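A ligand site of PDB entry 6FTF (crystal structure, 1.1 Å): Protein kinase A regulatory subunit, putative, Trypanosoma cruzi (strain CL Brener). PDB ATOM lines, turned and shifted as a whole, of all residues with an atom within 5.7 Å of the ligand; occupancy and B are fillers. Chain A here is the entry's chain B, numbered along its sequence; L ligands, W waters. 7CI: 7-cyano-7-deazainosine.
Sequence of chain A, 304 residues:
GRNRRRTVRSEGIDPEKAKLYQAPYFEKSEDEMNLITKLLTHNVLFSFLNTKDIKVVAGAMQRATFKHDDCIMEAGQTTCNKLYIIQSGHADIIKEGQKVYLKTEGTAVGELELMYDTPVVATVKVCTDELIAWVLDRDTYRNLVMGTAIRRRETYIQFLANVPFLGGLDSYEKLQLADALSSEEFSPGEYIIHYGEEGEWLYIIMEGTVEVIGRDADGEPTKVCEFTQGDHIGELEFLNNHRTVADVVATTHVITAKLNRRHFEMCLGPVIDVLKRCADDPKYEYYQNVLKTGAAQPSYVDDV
A nitrogen (N3) of the ligand lies within hydrogen-bond range of the backbone carbonyl oxygen (O) of Lys 283, 2.7 Å away. The side-chain carboxylate (OE1) of Glu 237 lies within hydrogen-bond range of an oxygen (O3) of the ligand (2.7 Å). The backbone NH (N) of Gly 234 is in hydrogen-bond range of an oxygen (O2) of the ligand, 3.0 Å away. O5 of the ligand is in hydrogen-bond range of N of Tyr 287 (3.0 Å). An oxygen (O3) of the ligand lies within hydrogen-bond range of the backbone NH (N) of Leu 236, 3.3 Å away. An oxygen (O4) of the ligand sits at hydrogen-bond distance from the backbone NH (N) of Ala 246, 3.3 Å away. O4 of the ligand lies within hydrogen-bond range of N of Val 245, at 3.3 Å. O3 of the ligand is in hydrogen-bond range of N of Glu 235 (3.4 Å).
Val 212 touches the ligand (CG1 to C2, 3.6 Å). Val 224 touches the ligand. SG of Cys 225 touches C3 of the ligand, 3.6 Å away. Phe 227 touches the ligand. Ile 233 touches the ligand. Val 248 touches the ligand (CG2 to O1, 3.5 Å). Tyr 284 touches the ligand. Tyr 286 touches the ligand (CD2 to N4, 3.1 Å). Val 290 touches the ligand. Hydrophobic or aromatic side chains within 4 Å of the ligand: Val 212, Val 224, Phe 227, Ile 233, Leu 236, Val 245, Ala 246, Val 248, Tyr 284, Tyr 286, Tyr 287 and Val 290.
The backbone NH (N) of Val 245 is in hydrogen-bond range of the side-chain carboxylate (OE2) of Glu 237 (3.5 Å). A ring nitrogen (ND1) of His 232 sits at hydrogen-bond distance from the side-chain carboxylate of Glu 235 (2.8 Å). O of Tyr 284 is in hydrogen-bond range of NE2 of Gln 288. The backbone NH (N) of Val 248 is in hydrogen-bond range of the backbone carbonyl oxygen (O) of Ile 193 (2.9 Å). N of Val 212 sits at hydrogen-bond distance from O of Cys 225 (2.9 Å). The backbone NH of Val 224 lies within hydrogen-bond range of the backbone carbonyl oxygen of Val 212 (2.8 Å).
Water W1 lies within hydrogen-bond range of OH of Tyr 284 (2.6 Å), OE2 of Glu 235 (2.7 Å), O2 of the ligand (2.8 Å) and O of His 232 (2.9 Å).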
ATOM      1  N   ILE A 193      -4.411 -22.460  -2.100  1.00  0.00           N
ATOM      2  CA  ILE A 193      -5.589 -22.502  -1.257  1.00  0.00           C
ATOM      3  C   ILE A 193      -6.785 -22.095  -2.110  1.00  0.00           C
ATOM      4  O   ILE A 193      -6.714 -21.134  -2.870  1.00  0.00           O
ATOM      5  CB  ILE A 193      -5.444 -21.569  -0.030  1.00  0.00           C
ATOM      6  CG1 ILE A 193      -4.323 -22.064   0.850  1.00  0.00           C
ATOM      7  CG2 ILE A 193      -6.764 -21.463   0.727  1.00  0.00           C
ATOM      8  CD1 ILE A 193      -3.897 -21.084   1.984  1.00  0.00           C
ATOM      9  N   VAL A 212      -3.554 -13.223  -3.494  1.00  0.00           N
ATOM     10  CA  VAL A 212      -4.673 -13.536  -2.612  1.00  0.00           C
ATOM     11  C   VAL A 212      -5.913 -12.936  -3.263  1.00  0.00           C
ATOM     12  O   VAL A 212      -5.921 -11.758  -3.593  1.00  0.00           O
ATOM     13  CB  VAL A 212      -4.445 -12.927  -1.222  1.00  0.00           C
ATOM     14  CG1 VAL A 212      -5.611 -13.201  -0.304  1.00  0.00           C
ATOM     15  CG2 VAL A 212      -3.176 -13.459  -0.595  1.00  0.00           C
ATOM     16  N   VAL A 224      -6.743  -9.101  -3.624  1.00  0.00           N
ATOM     17  CA  VAL A 224      -6.487  -8.398  -2.369  1.00  0.00           C
ATOM     18  C   VAL A 224      -5.050  -7.912  -2.276  1.00  0.00           C
ATOM     19  O   VAL A 224      -4.800  -6.745  -1.957  1.00  0.00           O
ATOM     20  CB  VAL A 224      -6.840  -9.332  -1.202  1.00  0.00           C
ATOM     21  CG1 VAL A 224      -6.457  -8.712   0.128  1.00  0.00           C
ATOM     22  CG2 VAL A 224      -8.319  -9.630  -1.204  1.00  0.00           C
ATOM     23  N   CYS A 225      -4.084  -8.780  -2.537  1.00  0.00           N
ATOM     24  CA  CYS A 225      -2.673  -8.434  -2.401  1.00  0.00           C
ATOM     25  C   CYS A 225      -1.834  -9.576  -2.959  1.00  0.00           C
ATOM     26  O   CYS A 225      -2.359 -10.583  -3.431  1.00  0.00           O
ATOM     27  CB  CYS A 225      -2.292  -8.169  -0.941  1.00  0.00           C
ATOM     28  SG  CYS A 225      -2.287  -9.626   0.148  1.00  0.00           S
ATOM     29  N   PHE A 227       1.955 -11.898  -1.971  1.00  0.00           N
ATOM     30  CA  PHE A 227       2.988 -12.277  -1.008  1.00  0.00           C
ATOM     31  C   PHE A 227       4.101 -12.962  -1.789  1.00  0.00           C
ATOM     32  O   PHE A 227       3.909 -13.440  -2.909  1.00  0.00           O
ATOM     33  CB  PHE A 227       2.448 -13.217   0.074  1.00  0.00           C
ATOM     34  CG  PHE A 227       1.513 -12.560   1.039  1.00  0.00           C
ATOM     35  CD1 PHE A 227       1.949 -11.554   1.883  1.00  0.00           C
ATOM     36  CD2 PHE A 227       0.204 -12.961   1.137  1.00  0.00           C
ATOM     37  CE1 PHE A 227       1.084 -10.949   2.775  1.00  0.00           C
ATOM     38  CE2 PHE A 227      -0.655 -12.368   2.040  1.00  0.00           C
ATOM     39  CZ  PHE A 227      -0.205 -11.364   2.855  1.00  0.00           C
ATOM     40  N   HIS A 232       4.051 -15.991   4.605  1.00  0.00           N
ATOM     41  CA  HIS A 232       3.237 -17.165   4.907  1.00  0.00           C
ATOM     42  C   HIS A 232       1.776 -16.916   4.580  1.00  0.00           C
ATOM     43  O   HIS A 232       1.286 -15.789   4.629  1.00  0.00           O
ATOM     44  CB  HIS A 232       3.334 -17.517   6.393  1.00  0.00           C
ATOM     45  CG  HIS A 232       3.101 -16.340   7.284  1.00  0.00           C
ATOM     46  ND1 HIS A 232       1.837 -15.917   7.654  1.00  0.00           N
ATOM     47  CD2 HIS A 232       3.965 -15.440   7.818  1.00  0.00           C
ATOM     48  CE1 HIS A 232       1.944 -14.825   8.397  1.00  0.00           C
ATOM     49  NE2 HIS A 232       3.221 -14.532   8.523  1.00  0.00           N
ATOM     50  N   ILE A 233       1.069 -18.006   4.263  1.00  0.00           N
ATOM     51  CA  ILE A 233      -0.374 -17.982   4.043  1.00  0.00           C
ATOM     52  C   ILE A 233      -1.005 -19.186   4.722  1.00  0.00           C
ATOM     53  O   ILE A 233      -0.348 -20.218   4.910  1.00  0.00           O
ATOM     54  CB  ILE A 233      -0.803 -17.927   2.545  1.00  0.00           C
ATOM     55  CG1 ILE A 233      -0.277 -19.130   1.742  1.00  0.00           C
ATOM     56  CG2 ILE A 233      -0.416 -16.581   1.919  1.00  0.00           C
ATOM     57  CD1 ILE A 233       1.026 -18.895   0.982  1.00  0.00           C
ATOM     58  N   GLY A 234      -2.269 -19.040   5.104  1.00  0.00           N
ATOM     59  CA  GLY A 234      -3.046 -20.107   5.717  1.00  0.00           C
ATOM     60  C   GLY A 234      -3.250 -19.954   7.198  1.00  0.00           C
ATOM     61  O   GLY A 234      -4.046 -20.698   7.788  1.00  0.00           O
ATOM     62  N   GLU A 235      -2.603 -18.993   7.847  1.00  0.00           N
ATOM     63  CA  GLU A 235      -2.694 -18.912   9.290  1.00  0.00           C
ATOM     64  C   GLU A 235      -4.016 -18.319   9.768  1.00  0.00           C
ATOM     65  O   GLU A 235      -4.377 -18.544  10.935  1.00  0.00           O
ATOM     66  CB  GLU A 235      -1.550 -18.106   9.898  1.00  0.00           C
ATOM     67  CG  GLU A 235      -1.626 -16.604   9.700  1.00  0.00           C
ATOM     68  CD  GLU A 235      -1.248 -16.145   8.320  1.00  0.00           C
ATOM     69  OE1 GLU A 235      -0.760 -16.971   7.503  1.00  0.00           O
ATOM     70  OE2 GLU A 235      -1.439 -14.921   8.058  1.00  0.00           O
ATOM     71  N   LEU A 236      -4.734 -17.555   8.949  1.00  0.00           N
ATOM     72  CA  LEU A 236      -5.881 -16.828   9.495  1.00  0.00           C
ATOM     73  C   LEU A 236      -6.957 -17.792   9.960  1.00  0.00           C
ATOM     74  O   LEU A 236      -7.565 -17.600  11.026  1.00  0.00           O
ATOM     75  CB  LEU A 236      -6.469 -15.885   8.445  1.00  0.00           C
ATOM     76  CG  LEU A 236      -5.533 -14.786   7.945  1.00  0.00           C
ATOM     77  CD1 LEU A 236      -6.263 -13.878   6.977  1.00  0.00           C
ATOM     78  CD2 LEU A 236      -4.949 -13.963   9.095  1.00  0.00           C
ATOM     79  N   GLU A 237      -7.195 -18.834   9.192  1.00  0.00           N
ATOM     80  CA  GLU A 237      -8.185 -19.842   9.557  1.00  0.00           C
ATOM     81  C   GLU A 237      -7.804 -20.560  10.838  1.00  0.00           C
ATOM     82  O   GLU A 237      -8.685 -20.988  11.597  1.00  0.00           O
ATOM     83  CB  GLU A 237      -8.326 -20.842   8.419  1.00  0.00           C
ATOM     84  CG  GLU A 237      -8.955 -20.256   7.153  1.00  0.00           C
ATOM     85  CD  GLU A 237      -8.103 -19.258   6.396  1.00  0.00           C
ATOM     86  OE1 GLU A 237      -6.854 -19.430   6.334  1.00  0.00           O
ATOM     87  OE2 GLU A 237      -8.664 -18.287   5.835  1.00  0.00           O
ATOM     88  N   THR A 244     -11.646 -21.163   4.793  1.00  0.00           N
ATOM     89  CA  THR A 244     -10.817 -20.213   4.062  1.00  0.00           C
ATOM     90  C   THR A 244     -11.661 -19.134   3.397  1.00  0.00           C
ATOM     91  O   THR A 244     -12.735 -19.405   2.843  1.00  0.00           O
ATOM     92  CB  THR A 244      -9.927 -20.919   3.039  1.00  0.00           C
ATOM     93  OG1 THR A 244     -10.753 -21.622   2.133  1.00  0.00           O
ATOM     94  CG2 THR A 244      -8.941 -21.874   3.697  1.00  0.00           C
ATOM     95  N   VAL A 245     -11.164 -17.913   3.478  1.00  0.00           N
ATOM     96  CA  VAL A 245     -11.867 -16.733   3.026  1.00  0.00           C
ATOM     97  C   VAL A 245     -11.246 -16.119   1.793  1.00  0.00           C
ATOM     98  O   VAL A 245     -11.709 -15.062   1.339  1.00  0.00           O
ATOM     99  CB  VAL A 245     -12.013 -15.713   4.176  1.00  0.00           C
ATOM    100  CG1 VAL A 245     -13.008 -16.224   5.200  1.00  0.00           C
ATOM    101  CG2 VAL A 245     -10.665 -15.478   4.866  1.00  0.00           C
ATOM    102  N   ALA A 246     -10.221 -16.747   1.234  1.00  0.00           N
ATOM    103  CA  ALA A 246      -9.620 -16.272  -0.004  1.00  0.00           C
ATOM    104  C   ALA A 246      -8.983 -17.442  -0.731  1.00  0.00           C
ATOM    105  O   ALA A 246      -8.599 -18.431  -0.104  1.00  0.00           O
ATOM    106  CB  ALA A 246      -8.536 -15.229   0.270  1.00  0.00           C
ATOM    107  N   ASP A 247      -8.881 -17.307  -2.046  1.00  0.00           N
ATOM    108  CA  ASP A 247      -7.983 -18.162  -2.810  1.00  0.00           C
ATOM    109  C   ASP A 247      -6.570 -17.613  -2.658  1.00  0.00           C
ATOM    110  O   ASP A 247      -6.368 -16.403  -2.545  1.00  0.00           O
ATOM    111  CB  ASP A 247      -8.326 -18.127  -4.287  1.00  0.00           C
ATOM    112  CG  ASP A 247      -9.762 -18.489  -4.588  1.00  0.00           C
ATOM    113  OD1 ASP A 247     -10.165 -19.619  -4.271  1.00  0.00           O
ATOM    114  OD2 ASP A 247     -10.479 -17.645  -5.193  1.00  0.00           O
ATOM    115  N   VAL A 248      -5.587 -18.494  -2.755  1.00  0.00           N
ATOM    116  CA  VAL A 248      -4.192 -18.098  -2.893  1.00  0.00           C
ATOM    117  C   VAL A 248      -3.655 -18.830  -4.104  1.00  0.00           C
ATOM    118  O   VAL A 248      -3.705 -20.066  -4.157  1.00  0.00           O
ATOM    119  CB  VAL A 248      -3.358 -18.420  -1.641  1.00  0.00           C
ATOM    120  CG1 VAL A 248      -1.945 -17.942  -1.865  1.00  0.00           C
ATOM    121  CG2 VAL A 248      -3.988 -17.772  -0.414  1.00  0.00           C
ATOM    122  N   LYS A 283      -2.404  -4.736   4.270  1.00  0.00           N
ATOM    123  CA  LYS A 283      -2.708  -5.806   3.331  1.00  0.00           C
ATOM    124  C   LYS A 283      -3.851  -6.694   3.801  1.00  0.00           C
ATOM    125  O   LYS A 283      -4.386  -7.466   3.001  1.00  0.00           O
ATOM    126  CB  LYS A 283      -1.468  -6.659   3.047  1.00  0.00           C
ATOM    127  CG  LYS A 283      -0.364  -5.883   2.357  1.00  0.00           C
ATOM    128  CD  LYS A 283       0.975  -6.627   2.301  1.00  0.00           C
ATOM    129  CE  LYS A 283       1.068  -7.582   1.105  1.00  0.00           C
ATOM    130  NZ  LYS A 283       2.491  -7.979   0.746  1.00  0.00           N
ATOM    131  N   TYR A 284      -4.238  -6.593   5.084  1.00  0.00           N
ATOM    132  CA  TYR A 284      -5.320  -7.377   5.665  1.00  0.00           C
ATOM    133  C   TYR A 284      -6.566  -6.544   5.959  1.00  0.00           C
ATOM    134  O   TYR A 284      -7.439  -6.993   6.698  1.00  0.00           O
ATOM    135  CB  TYR A 284      -4.847  -8.124   6.907  1.00  0.00           C
ATOM    136  CG  TYR A 284      -3.744  -9.155   6.660  1.00  0.00           C
ATOM    137  CD1 TYR A 284      -2.426  -8.770   6.461  1.00  0.00           C
ATOM    138  CD2 TYR A 284      -4.039 -10.503   6.632  1.00  0.00           C
ATOM    139  CE1 TYR A 284      -1.441  -9.715   6.231  1.00  0.00           C
ATOM    140  CE2 TYR A 284      -3.054 -11.449   6.412  1.00  0.00           C
ATOM    141  CZ  TYR A 284      -1.756 -11.051   6.221  1.00  0.00           C
ATOM    142  OH  TYR A 284      -0.739 -11.951   5.986  1.00  0.00           O
ATOM    143  N   GLU A 285      -6.692  -5.365   5.341  1.00  0.00           N
ATOM    144  CA  GLU A 285      -7.909  -4.580   5.486  1.00  0.00           C
ATOM    145  C   GLU A 285      -9.133  -5.378   5.038  1.00  0.00           C
ATOM    146  O   GLU A 285     -10.177  -5.345   5.688  1.00  0.00           O
ATOM    147  CB  GLU A 285      -7.789  -3.289   4.671  1.00  0.00           C
ATOM    148  CG  GLU A 285      -9.009  -2.399   4.778  1.00  0.00           C
ATOM    149  CD  GLU A 285      -8.862  -1.078   4.049  1.00  0.00           C
ATOM    150  OE1 GLU A 285      -9.835  -0.296   4.054  1.00  0.00           O
ATOM    151  OE2 GLU A 285      -7.774  -0.827   3.473  1.00  0.00           O
ATOM    152  N   TYR A 286      -9.025  -6.085   3.922  1.00  0.00           N
ATOM    153  CA  TYR A 286     -10.126  -6.907   3.430  1.00  0.00           C
ATOM    154  C   TYR A 286     -10.567  -7.919   4.503  1.00  0.00           C
ATOM    155  O   TYR A 286     -11.757  -8.049   4.796  1.00  0.00           O
ATOM    156  CB  TYR A 286      -9.692  -7.601   2.125  1.00  0.00           C
ATOM    157  CG  TYR A 286     -10.713  -8.583   1.619  1.00  0.00           C
ATOM    158  CD1 TYR A 286     -11.739  -8.192   0.788  1.00  0.00           C
ATOM    159  CD2 TYR A 286     -10.649  -9.898   2.002  1.00  0.00           C
ATOM    160  CE1 TYR A 286     -12.696  -9.079   0.353  1.00  0.00           C
ATOM    161  CE2 TYR A 286     -11.602 -10.807   1.578  1.00  0.00           C
ATOM    162  CZ  TYR A 286     -12.613 -10.390   0.750  1.00  0.00           C
ATOM    163  OH  TYR A 286     -13.582 -11.275   0.334  1.00  0.00           O
ATOM    164  N   TYR A 287      -9.611  -8.619   5.103  1.00  0.00           N
ATOM    165  CA  TYR A 287      -9.937  -9.611   6.121  1.00  0.00           C
ATOM    166  C   TYR A 287     -10.608  -8.973   7.322  1.00  0.00           C
ATOM    167  O   TYR A 287     -11.498  -9.584   7.914  1.00  0.00           O
ATOM    168  CB  TYR A 287      -8.664 -10.309   6.582  1.00  0.00           C
ATOM    169  CG  TYR A 287      -8.889 -11.396   7.610  1.00  0.00           C
ATOM    170  CD1 TYR A 287      -9.707 -12.495   7.339  1.00  0.00           C
ATOM    171  CD2 TYR A 287      -8.249 -11.356   8.826  1.00  0.00           C
ATOM    172  CE1 TYR A 287      -9.873 -13.516   8.256  1.00  0.00           C
ATOM    173  CE2 TYR A 287      -8.381 -12.364   9.748  1.00  0.00           C
ATOM    174  CZ  TYR A 287      -9.202 -13.442   9.457  1.00  0.00           C
ATOM    175  OH  TYR A 287      -9.315 -14.444  10.392  1.00  0.00           O
ATOM    176  N   GLN A 288     -10.185  -7.775   7.716  1.00  0.00           N
ATOM    177  CA  GLN A 288     -10.830  -7.149   8.860  1.00  0.00           C
ATOM    178  C   GLN A 288     -12.318  -6.980   8.597  1.00  0.00           C
ATOM    179  O   GLN A 288     -13.132  -7.104   9.516  1.00  0.00           O
ATOM    180  CB  GLN A 288     -10.229  -5.781   9.191  1.00  0.00           C
ATOM    181  CG  GLN A 288      -8.753  -5.746   9.498  1.00  0.00           C
ATOM    182  CD  GLN A 288      -8.299  -6.905  10.331  1.00  0.00           C
ATOM    183  OE1 GLN A 288      -8.740  -7.090  11.458  1.00  0.00           O
ATOM    184  NE2 GLN A 288      -7.372  -7.687   9.785  1.00  0.00           N
ATOM    185  N   VAL A 290     -14.120  -8.924   6.537  1.00  0.00           N
ATOM    186  CA  VAL A 290     -14.686 -10.263   6.635  1.00  0.00           C
ATOM    187  C   VAL A 290     -15.057 -10.563   8.071  1.00  0.00           C
ATOM    188  O   VAL A 290     -16.148 -11.083   8.366  1.00  0.00           O
ATOM    189  CB  VAL A 290     -13.673 -11.299   6.103  1.00  0.00           C
ATOM    190  CG1 VAL A 290     -14.120 -12.717   6.427  1.00  0.00           C
ATOM    191  CG2 VAL A 290     -13.511 -11.177   4.625  1.00  0.00           C
HETATM  192  C1  7CI L   1      -4.718 -15.187   3.137  1.00  0.00           C
HETATM  193  N1  7CI L   1      -5.661 -14.009   3.268  1.00  0.00           N
HETATM  194  O1  7CI L   1      -5.371 -16.237   2.455  1.00  0.00           O
HETATM  195  C2  7CI L   1      -5.279 -12.749   3.265  1.00  0.00           C
HETATM  196  N2  7CI L   1      -4.033 -12.230   3.131  1.00  0.00           N
HETATM  197  O2  7CI L   1      -3.054 -16.253   4.436  1.00  0.00           O
HETATM  198  C3  7CI L   1      -3.905 -10.892   3.076  1.00  0.00           C
HETATM  199  N3  7CI L   1      -5.021 -10.049   3.256  1.00  0.00           N
HETATM  200  O3  7CI L   1      -4.896 -17.712   5.684  1.00  0.00           O
HETATM  201  C4  7CI L   1      -6.281 -10.557   3.438  1.00  0.00           C
HETATM  202  N4  7CI L   1     -10.066 -12.344   3.895  1.00  0.00           N
HETATM  203  C5  7CI L   1      -6.454 -11.954   3.425  1.00  0.00           C
HETATM  204  O5  7CI L   1      -7.206  -9.726   3.643  1.00  0.00           O
HETATM  205  C6  7CI L   1      -7.588 -12.874   3.521  1.00  0.00           C
HETATM  206  C7  7CI L   1      -7.014 -14.127   3.399  1.00  0.00           C
HETATM  207  C8  7CI L   1      -8.940 -12.575   3.725  1.00  0.00           C
HETATM  208  C9  7CI L   1      -4.335 -15.734   4.463  1.00  0.00           C
HETATM  209  C10 7CI L   1      -5.341 -16.741   4.695  1.00  0.00           C
HETATM  210  C11 7CI L   1      -5.452 -17.385   3.299  1.00  0.00           C
HETATM  211  C12 7CI L   1      -6.823 -18.131   3.036  1.00  0.00           C
HETATM  212  O4  7CI L   1      -7.876 -17.345   3.444  1.00  0.00           O
HETATM  213  O   HOH W   1      -1.154 -14.505   5.454  1.00  0.00           O
